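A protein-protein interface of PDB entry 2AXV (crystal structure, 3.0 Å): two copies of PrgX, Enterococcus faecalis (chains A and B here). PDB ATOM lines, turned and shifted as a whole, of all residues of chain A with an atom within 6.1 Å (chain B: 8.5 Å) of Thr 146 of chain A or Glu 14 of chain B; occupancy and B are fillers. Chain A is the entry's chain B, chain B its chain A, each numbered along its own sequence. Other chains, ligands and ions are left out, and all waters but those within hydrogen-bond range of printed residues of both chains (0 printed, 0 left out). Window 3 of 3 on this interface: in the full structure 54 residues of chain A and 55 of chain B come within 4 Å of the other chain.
Thr 146 of chain A touches just one residue of chain B: Glu 14 (2.9 Å).
Phe 148 of chain A touches none of the printed residues of chain B.
Of the printed residues of chain B, Phe 149 of chain A touches Ile 11 and Val 56.
Of the printed residues of chain A, Ile 11 of chain B touches Phe 149 (3.8 Å).
Glu 14 of chain B touches three residues of chain A.
Printed residues of chain A within 4 Å of Leu 15 of chain B: Arg 145.
Asn 16 of chain B touches none of the printed residues of chain A.
Printed residues of chain A within 4 Å of Val 56 of chain B: Phe 149 (3.7 Å).
No position is printed for both chains.
The backbone carbonyl oxygen (O) of Thr 147 of chain A sits at hydrogen-bond distance from the guanidinium group (NH2) of Arg 145 of chain A (2.8 Å).
Arg 145 of chain A touches Leu 15 of chain B (CZ to CD1, 3.6 Å).
CZ of Phe 149 of chain A touches CG1 of Ile 11 of chain B (3.8 Å).
Phe 149 of chain A touches Val 56 of chain B (CD1 to CG1, 3.7 Å).
N of Thr 147 of chain A sits at hydrogen-bond distance from OE1 of Glu 14 of chain B (3.0 Å).
The guanidinium group (NE) of Arg 145 of chain A lies within salt-bridge range of the side-chain carboxylate (OE1) of Glu 14 of chain B, 2.9 Å away.
N of Thr 146 of chain A sits at hydrogen-bond distance from OE1 of Glu 14 of chain B, at 2.9 Å.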
ATOM      1  N   LYS A 144      23.451   9.792   8.997  1.00  0.00           N
ATOM      2  CA  LYS A 144      22.865  10.930   8.286  1.00  0.00           C
ATOM      3  C   LYS A 144      21.422  10.666   7.882  1.00  0.00           C
ATOM      4  O   LYS A 144      21.014  10.947   6.752  1.00  0.00           O
ATOM      5  CB  LYS A 144      23.799  11.340   7.115  1.00  0.00           C
ATOM      6  CG  LYS A 144      24.589  12.675   7.413  1.00  0.00           C
ATOM      7  CD  LYS A 144      26.133  12.575   7.324  1.00  0.00           C
ATOM      8  CE  LYS A 144      26.683  13.045   5.969  1.00  0.00           C
ATOM      9  NZ  LYS A 144      26.344  12.058   4.883  1.00  0.00           N
ATOM     10  N   ARG A 145      20.659  10.113   8.820  1.00  0.00           N
ATOM     11  CA  ARG A 145      19.287   9.705   8.556  1.00  0.00           C
ATOM     12  C   ARG A 145      18.326  10.605   9.279  1.00  0.00           C
ATOM     13  O   ARG A 145      18.530  10.931  10.442  1.00  0.00           O
ATOM     14  CB  ARG A 145      19.051   8.271   8.981  1.00  0.00           C
ATOM     15  CG  ARG A 145      19.555   7.300   7.963  1.00  0.00           C
ATOM     16  CD  ARG A 145      18.716   7.314   6.702  1.00  0.00           C
ATOM     17  NE  ARG A 145      17.344   6.864   6.971  1.00  0.00           N
ATOM     18  CZ  ARG A 145      16.989   5.590   7.156  1.00  0.00           C
ATOM     19  NH1 ARG A 145      17.879   4.606   7.132  1.00  0.00           N
ATOM     20  NH2 ARG A 145      15.739   5.276   7.379  1.00  0.00           N
ATOM     21  N   THR A 146      17.247  10.969   8.593  1.00  0.00           N
ATOM     22  CA  THR A 146      16.237  11.848   9.178  1.00  0.00           C
ATOM     23  C   THR A 146      14.831  11.257   9.159  1.00  0.00           C
ATOM     24  O   THR A 146      14.047  11.594  10.007  1.00  0.00           O
ATOM     25  CB  THR A 146      16.215  13.226   8.539  1.00  0.00           C
ATOM     26  OG1 THR A 146      16.093  13.065   7.130  1.00  0.00           O
ATOM     27  CG2 THR A 146      17.482  13.969   8.865  1.00  0.00           C
ATOM     28  N   THR A 147      14.484  10.414   8.199  1.00  0.00           N
ATOM     29  CA  THR A 147      13.177   9.754   8.220  1.00  0.00           C
ATOM     30  C   THR A 147      13.370   8.234   8.310  1.00  0.00           C
ATOM     31  O   THR A 147      14.352   7.722   7.782  1.00  0.00           O
ATOM     32  CB  THR A 147      12.332  10.260   7.026  1.00  0.00           C
ATOM     33  OG1 THR A 147      11.919  11.611   7.316  1.00  0.00           O
ATOM     34  CG2 THR A 147      11.090   9.369   6.760  1.00  0.00           C
ATOM     35  N   PHE A 148      12.464   7.567   9.038  1.00  0.00           N
ATOM     36  CA  PHE A 148      12.566   6.156   9.356  1.00  0.00           C
ATOM     37  C   PHE A 148      11.306   5.343   9.010  1.00  0.00           C
ATOM     38  O   PHE A 148      10.172   5.789   9.118  1.00  0.00           O
ATOM     39  CB  PHE A 148      12.834   6.028  10.834  1.00  0.00           C
ATOM     40  CG  PHE A 148      14.009   6.812  11.290  1.00  0.00           C
ATOM     41  CD1 PHE A 148      13.853   8.064  11.818  1.00  0.00           C
ATOM     42  CD2 PHE A 148      15.284   6.296  11.188  1.00  0.00           C
ATOM     43  CE1 PHE A 148      14.937   8.761  12.237  1.00  0.00           C
ATOM     44  CE2 PHE A 148      16.366   7.009  11.616  1.00  0.00           C
ATOM     45  CZ  PHE A 148      16.193   8.229  12.134  1.00  0.00           C
ATOM     46  N   PHE A 149      11.530   4.104   8.638  1.00  0.00           N
ATOM     47  CA  PHE A 149      10.517   3.295   8.075  1.00  0.00           C
ATOM     48  C   PHE A 149      10.412   2.101   8.945  1.00  0.00           C
ATOM     49  O   PHE A 149      11.261   1.861   9.794  1.00  0.00           O
ATOM     50  CB  PHE A 149      10.932   2.962   6.668  1.00  0.00           C
ATOM     51  CG  PHE A 149      11.314   4.185   5.867  1.00  0.00           C
ATOM     52  CD1 PHE A 149      12.643   4.439   5.525  1.00  0.00           C
ATOM     53  CD2 PHE A 149      10.329   5.127   5.501  1.00  0.00           C
ATOM     54  CE1 PHE A 149      12.979   5.581   4.797  1.00  0.00           C
ATOM     55  CE2 PHE A 149      10.654   6.293   4.762  1.00  0.00           C
ATOM     56  CZ  PHE A 149      11.981   6.516   4.416  1.00  0.00           C
ATOM     57  N   PRO A 174      15.778   9.144  17.975  1.00  0.00           N
ATOM     58  CA  PRO A 174      15.314   9.895  16.781  1.00  0.00           C
ATOM     59  C   PRO A 174      14.065   9.369  16.004  1.00  0.00           C
ATOM     60  O   PRO A 174      13.456  10.130  15.243  1.00  0.00           O
ATOM     61  CB  PRO A 174      16.542   9.866  15.872  1.00  0.00           C
ATOM     62  CG  PRO A 174      17.392   8.740  16.412  1.00  0.00           C
ATOM     63  CD  PRO A 174      17.188   8.741  17.856  1.00  0.00           C
ATOM     64  N   VAL B   7       7.013   9.337  -3.625  1.00  0.00           N
ATOM     65  CA  VAL B   7       7.387   8.623  -2.412  1.00  0.00           C
ATOM     66  C   VAL B   7       8.627   7.772  -2.668  1.00  0.00           C
ATOM     67  O   VAL B   7       9.479   7.666  -1.795  1.00  0.00           O
ATOM     68  CB  VAL B   7       6.232   7.772  -1.872  1.00  0.00           C
ATOM     69  CG1 VAL B   7       6.681   6.930  -0.677  1.00  0.00           C
ATOM     70  CG2 VAL B   7       5.061   8.670  -1.469  1.00  0.00           C
ATOM     71  N   LEU B   8       8.736   7.180  -3.857  1.00  0.00           N
ATOM     72  CA  LEU B   8       9.953   6.496  -4.243  1.00  0.00           C
ATOM     73  C   LEU B   8      11.142   7.457  -4.207  1.00  0.00           C
ATOM     74  O   LEU B   8      12.170   7.097  -3.664  1.00  0.00           O
ATOM     75  CB  LEU B   8       9.817   5.851  -5.619  1.00  0.00           C
ATOM     76  CG  LEU B   8       8.922   4.607  -5.696  1.00  0.00           C
ATOM     77  CD1 LEU B   8       8.696   4.119  -7.161  1.00  0.00           C
ATOM     78  CD2 LEU B   8       9.479   3.463  -4.833  1.00  0.00           C
ATOM     79  N   LYS B   9      10.998   8.665  -4.761  1.00  0.00           N
ATOM     80  CA  LYS B   9      12.089   9.645  -4.754  1.00  0.00           C
ATOM     81  C   LYS B   9      12.489   9.948  -3.330  1.00  0.00           C
ATOM     82  O   LYS B   9      13.643   9.909  -2.984  1.00  0.00           O
ATOM     83  CB  LYS B   9      11.662  10.957  -5.455  1.00  0.00           C
ATOM     84  CG  LYS B   9      12.819  11.965  -5.768  1.00  0.00           C
ATOM     85  CD  LYS B   9      12.399  13.219  -6.619  1.00  0.00           C
ATOM     86  CE  LYS B   9      13.392  14.411  -6.410  1.00  0.00           C
ATOM     87  NZ  LYS B   9      12.963  15.696  -7.052  1.00  0.00           N
ATOM     88  N   GLN B  10      11.496  10.276  -2.528  1.00  0.00           N
ATOM     89  CA  GLN B  10      11.678  10.696  -1.154  1.00  0.00           C
ATOM     90  C   GLN B  10      12.477   9.669  -0.415  1.00  0.00           C
ATOM     91  O   GLN B  10      13.434   9.981   0.239  1.00  0.00           O
ATOM     92  CB  GLN B  10      10.276  10.862  -0.550  1.00  0.00           C
ATOM     93  CG  GLN B  10      10.099  11.254   0.940  1.00  0.00           C
ATOM     94  CD  GLN B  10       8.594  11.295   1.283  1.00  0.00           C
ATOM     95  OE1 GLN B  10       8.163  10.805   2.337  1.00  0.00           O
ATOM     96  NE2 GLN B  10       7.779  11.821   0.344  1.00  0.00           N
ATOM     97  N   ILE B  11      12.083   8.425  -0.556  1.00  0.00           N
ATOM     98  CA  ILE B  11      12.754   7.336   0.134  1.00  0.00           C
ATOM     99  C   ILE B  11      14.145   7.093  -0.439  1.00  0.00           C
ATOM    100  O   ILE B  11      15.077   6.809   0.295  1.00  0.00           O
ATOM    101  CB  ILE B  11      11.901   6.022   0.104  1.00  0.00           C
ATOM    102  CG1 ILE B  11      10.593   6.246   0.898  1.00  0.00           C
ATOM    103  CG2 ILE B  11      12.676   4.819   0.674  1.00  0.00           C
ATOM    104  CD1 ILE B  11       9.480   5.252   0.582  1.00  0.00           C
ATOM    105  N   ARG B  12      14.282   7.201  -1.750  1.00  0.00           N
ATOM    106  CA  ARG B  12      15.568   6.972  -2.388  1.00  0.00           C
ATOM    107  C   ARG B  12      16.594   7.962  -1.870  1.00  0.00           C
ATOM    108  O   ARG B  12      17.672   7.579  -1.419  1.00  0.00           O
ATOM    109  CB  ARG B  12      15.466   7.088  -3.901  1.00  0.00           C
ATOM    110  CG  ARG B  12      16.603   6.452  -4.611  1.00  0.00           C
ATOM    111  CD  ARG B  12      16.583   6.760  -6.066  1.00  0.00           C
ATOM    112  NE  ARG B  12      17.347   7.986  -6.294  1.00  0.00           N
ATOM    113  CZ  ARG B  12      16.839   9.175  -6.572  1.00  0.00           C
ATOM    114  NH1 ARG B  12      15.529   9.347  -6.691  1.00  0.00           N
ATOM    115  NH2 ARG B  12      17.664  10.204  -6.742  1.00  0.00           N
ATOM    116  N   GLN B  13      16.239   9.239  -1.955  1.00  0.00           N
ATOM    117  CA  GLN B  13      17.106  10.309  -1.532  1.00  0.00           C
ATOM    118  C   GLN B  13      17.413  10.142  -0.063  1.00  0.00           C
ATOM    119  O   GLN B  13      18.553  10.259   0.331  1.00  0.00           O
ATOM    120  CB  GLN B  13      16.464  11.682  -1.812  1.00  0.00           C
ATOM    121  CG  GLN B  13      17.102  12.477  -2.960  1.00  0.00           C
ATOM    122  CD  GLN B  13      16.095  12.904  -4.020  1.00  0.00           C
ATOM    123  OE1 GLN B  13      15.563  12.053  -4.736  1.00  0.00           O
ATOM    124  NE2 GLN B  13      15.853  14.222  -4.152  1.00  0.00           N
ATOM    125  N   GLU B  14      16.407   9.845   0.751  1.00  0.00           N
ATOM    126  CA  GLU B  14      16.620   9.663   2.197  1.00  0.00           C
ATOM    127  C   GLU B  14      17.753   8.684   2.493  1.00  0.00           C
ATOM    128  O   GLU B  14      18.542   8.889   3.393  1.00  0.00           O
ATOM    129  CB  GLU B  14      15.331   9.147   2.848  1.00  0.00           C
ATOM    130  CG  GLU B  14      15.436   8.732   4.296  1.00  0.00           C
ATOM    131  CD  GLU B  14      15.983   9.832   5.174  1.00  0.00           C
ATOM    132  OE1 GLU B  14      16.583   9.522   6.226  1.00  0.00           O
ATOM    133  OE2 GLU B  14      15.793  11.012   4.828  1.00  0.00           O
ATOM    134  N   LEU B  15      17.804   7.615   1.713  1.00  0.00           N
ATOM    135  CA  LEU B  15      18.764   6.536   1.893  1.00  0.00           C
ATOM    136  C   LEU B  15      20.028   6.757   1.108  1.00  0.00           C
ATOM    137  O   LEU B  15      20.930   5.927   1.131  1.00  0.00           O
ATOM    138  CB  LEU B  15      18.150   5.222   1.424  1.00  0.00           C
ATOM    139  CG  LEU B  15      17.290   4.411   2.387  1.00  0.00           C
ATOM    140  CD1 LEU B  15      16.795   5.186   3.587  1.00  0.00           C
ATOM    141  CD2 LEU B  15      16.112   3.810   1.637  1.00  0.00           C
ATOM    142  N   ASN B  16      20.076   7.863   0.384  1.00  0.00           N
ATOM    143  CA  ASN B  16      21.204   8.201  -0.433  1.00  0.00           C
ATOM    144  C   ASN B  16      21.466   7.096  -1.463  1.00  0.00           C
ATOM    145  O   ASN B  16      22.580   6.574  -1.577  1.00  0.00           O
ATOM    146  CB  ASN B  16      22.421   8.463   0.468  1.00  0.00           C
ATOM    147  CG  ASN B  16      23.464   9.331  -0.213  1.00  0.00           C
ATOM    148  OD1 ASN B  16      24.366   8.826  -0.898  1.00  0.00           O
ATOM    149  ND2 ASN B  16      23.331  10.652  -0.058  1.00  0.00           N
ATOM    150  N   TYR B  17      20.411   6.729  -2.185  1.00  0.00           N
ATOM    151  CA  TYR B  17      20.555   5.946  -3.389  1.00  0.00           C
ATOM    152  C   TYR B  17      20.483   6.926  -4.565  1.00  0.00           C
ATOM    153  O   TYR B  17      19.969   8.056  -4.436  1.00  0.00           O
ATOM    154  CB  TYR B  17      19.418   4.939  -3.511  1.00  0.00           C
ATOM    155  CG  TYR B  17      19.477   3.695  -2.666  1.00  0.00           C
ATOM    156  CD1 TYR B  17      20.514   2.778  -2.791  1.00  0.00           C
ATOM    157  CD2 TYR B  17      18.439   3.385  -1.799  1.00  0.00           C
ATOM    158  CE1 TYR B  17      20.536   1.599  -2.020  1.00  0.00           C
ATOM    159  CE2 TYR B  17      18.452   2.223  -1.037  1.00  0.00           C
ATOM    160  CZ  TYR B  17      19.493   1.334  -1.147  1.00  0.00           C
ATOM    161  OH  TYR B  17      19.466   0.199  -0.373  1.00  0.00           O
ATOM    162  N   LEU B  54      15.098  -0.448  -2.158  1.00  0.00           N
ATOM    163  CA  LEU B  54      15.134   0.549  -1.104  1.00  0.00           C
ATOM    164  C   LEU B  54      15.271  -0.116   0.259  1.00  0.00           C
ATOM    165  O   LEU B  54      15.933   0.418   1.195  1.00  0.00           O
ATOM    166  CB  LEU B  54      13.850   1.347  -1.134  1.00  0.00           C
ATOM    167  CG  LEU B  54      13.720   2.104  -2.438  1.00  0.00           C
ATOM    168  CD1 LEU B  54      12.302   2.479  -2.593  1.00  0.00           C
ATOM    169  CD2 LEU B  54      14.620   3.323  -2.449  1.00  0.00           C
ATOM    170  N   VAL B  56      12.503  -0.802   2.032  1.00  0.00           N
ATOM    171  CA  VAL B  56      11.297  -0.537   2.824  1.00  0.00           C
ATOM    172  C   VAL B  56      10.150  -1.269   2.177  1.00  0.00           C
ATOM    173  O   VAL B  56      10.163  -1.573   1.007  1.00  0.00           O
ATOM    174  CB  VAL B  56      10.985   0.979   3.195  1.00  0.00           C
ATOM    175  CG1 VAL B  56      12.177   1.875   2.911  1.00  0.00           C
ATOM    176  CG2 VAL B  56       9.722   1.513   2.544  1.00  0.00           C
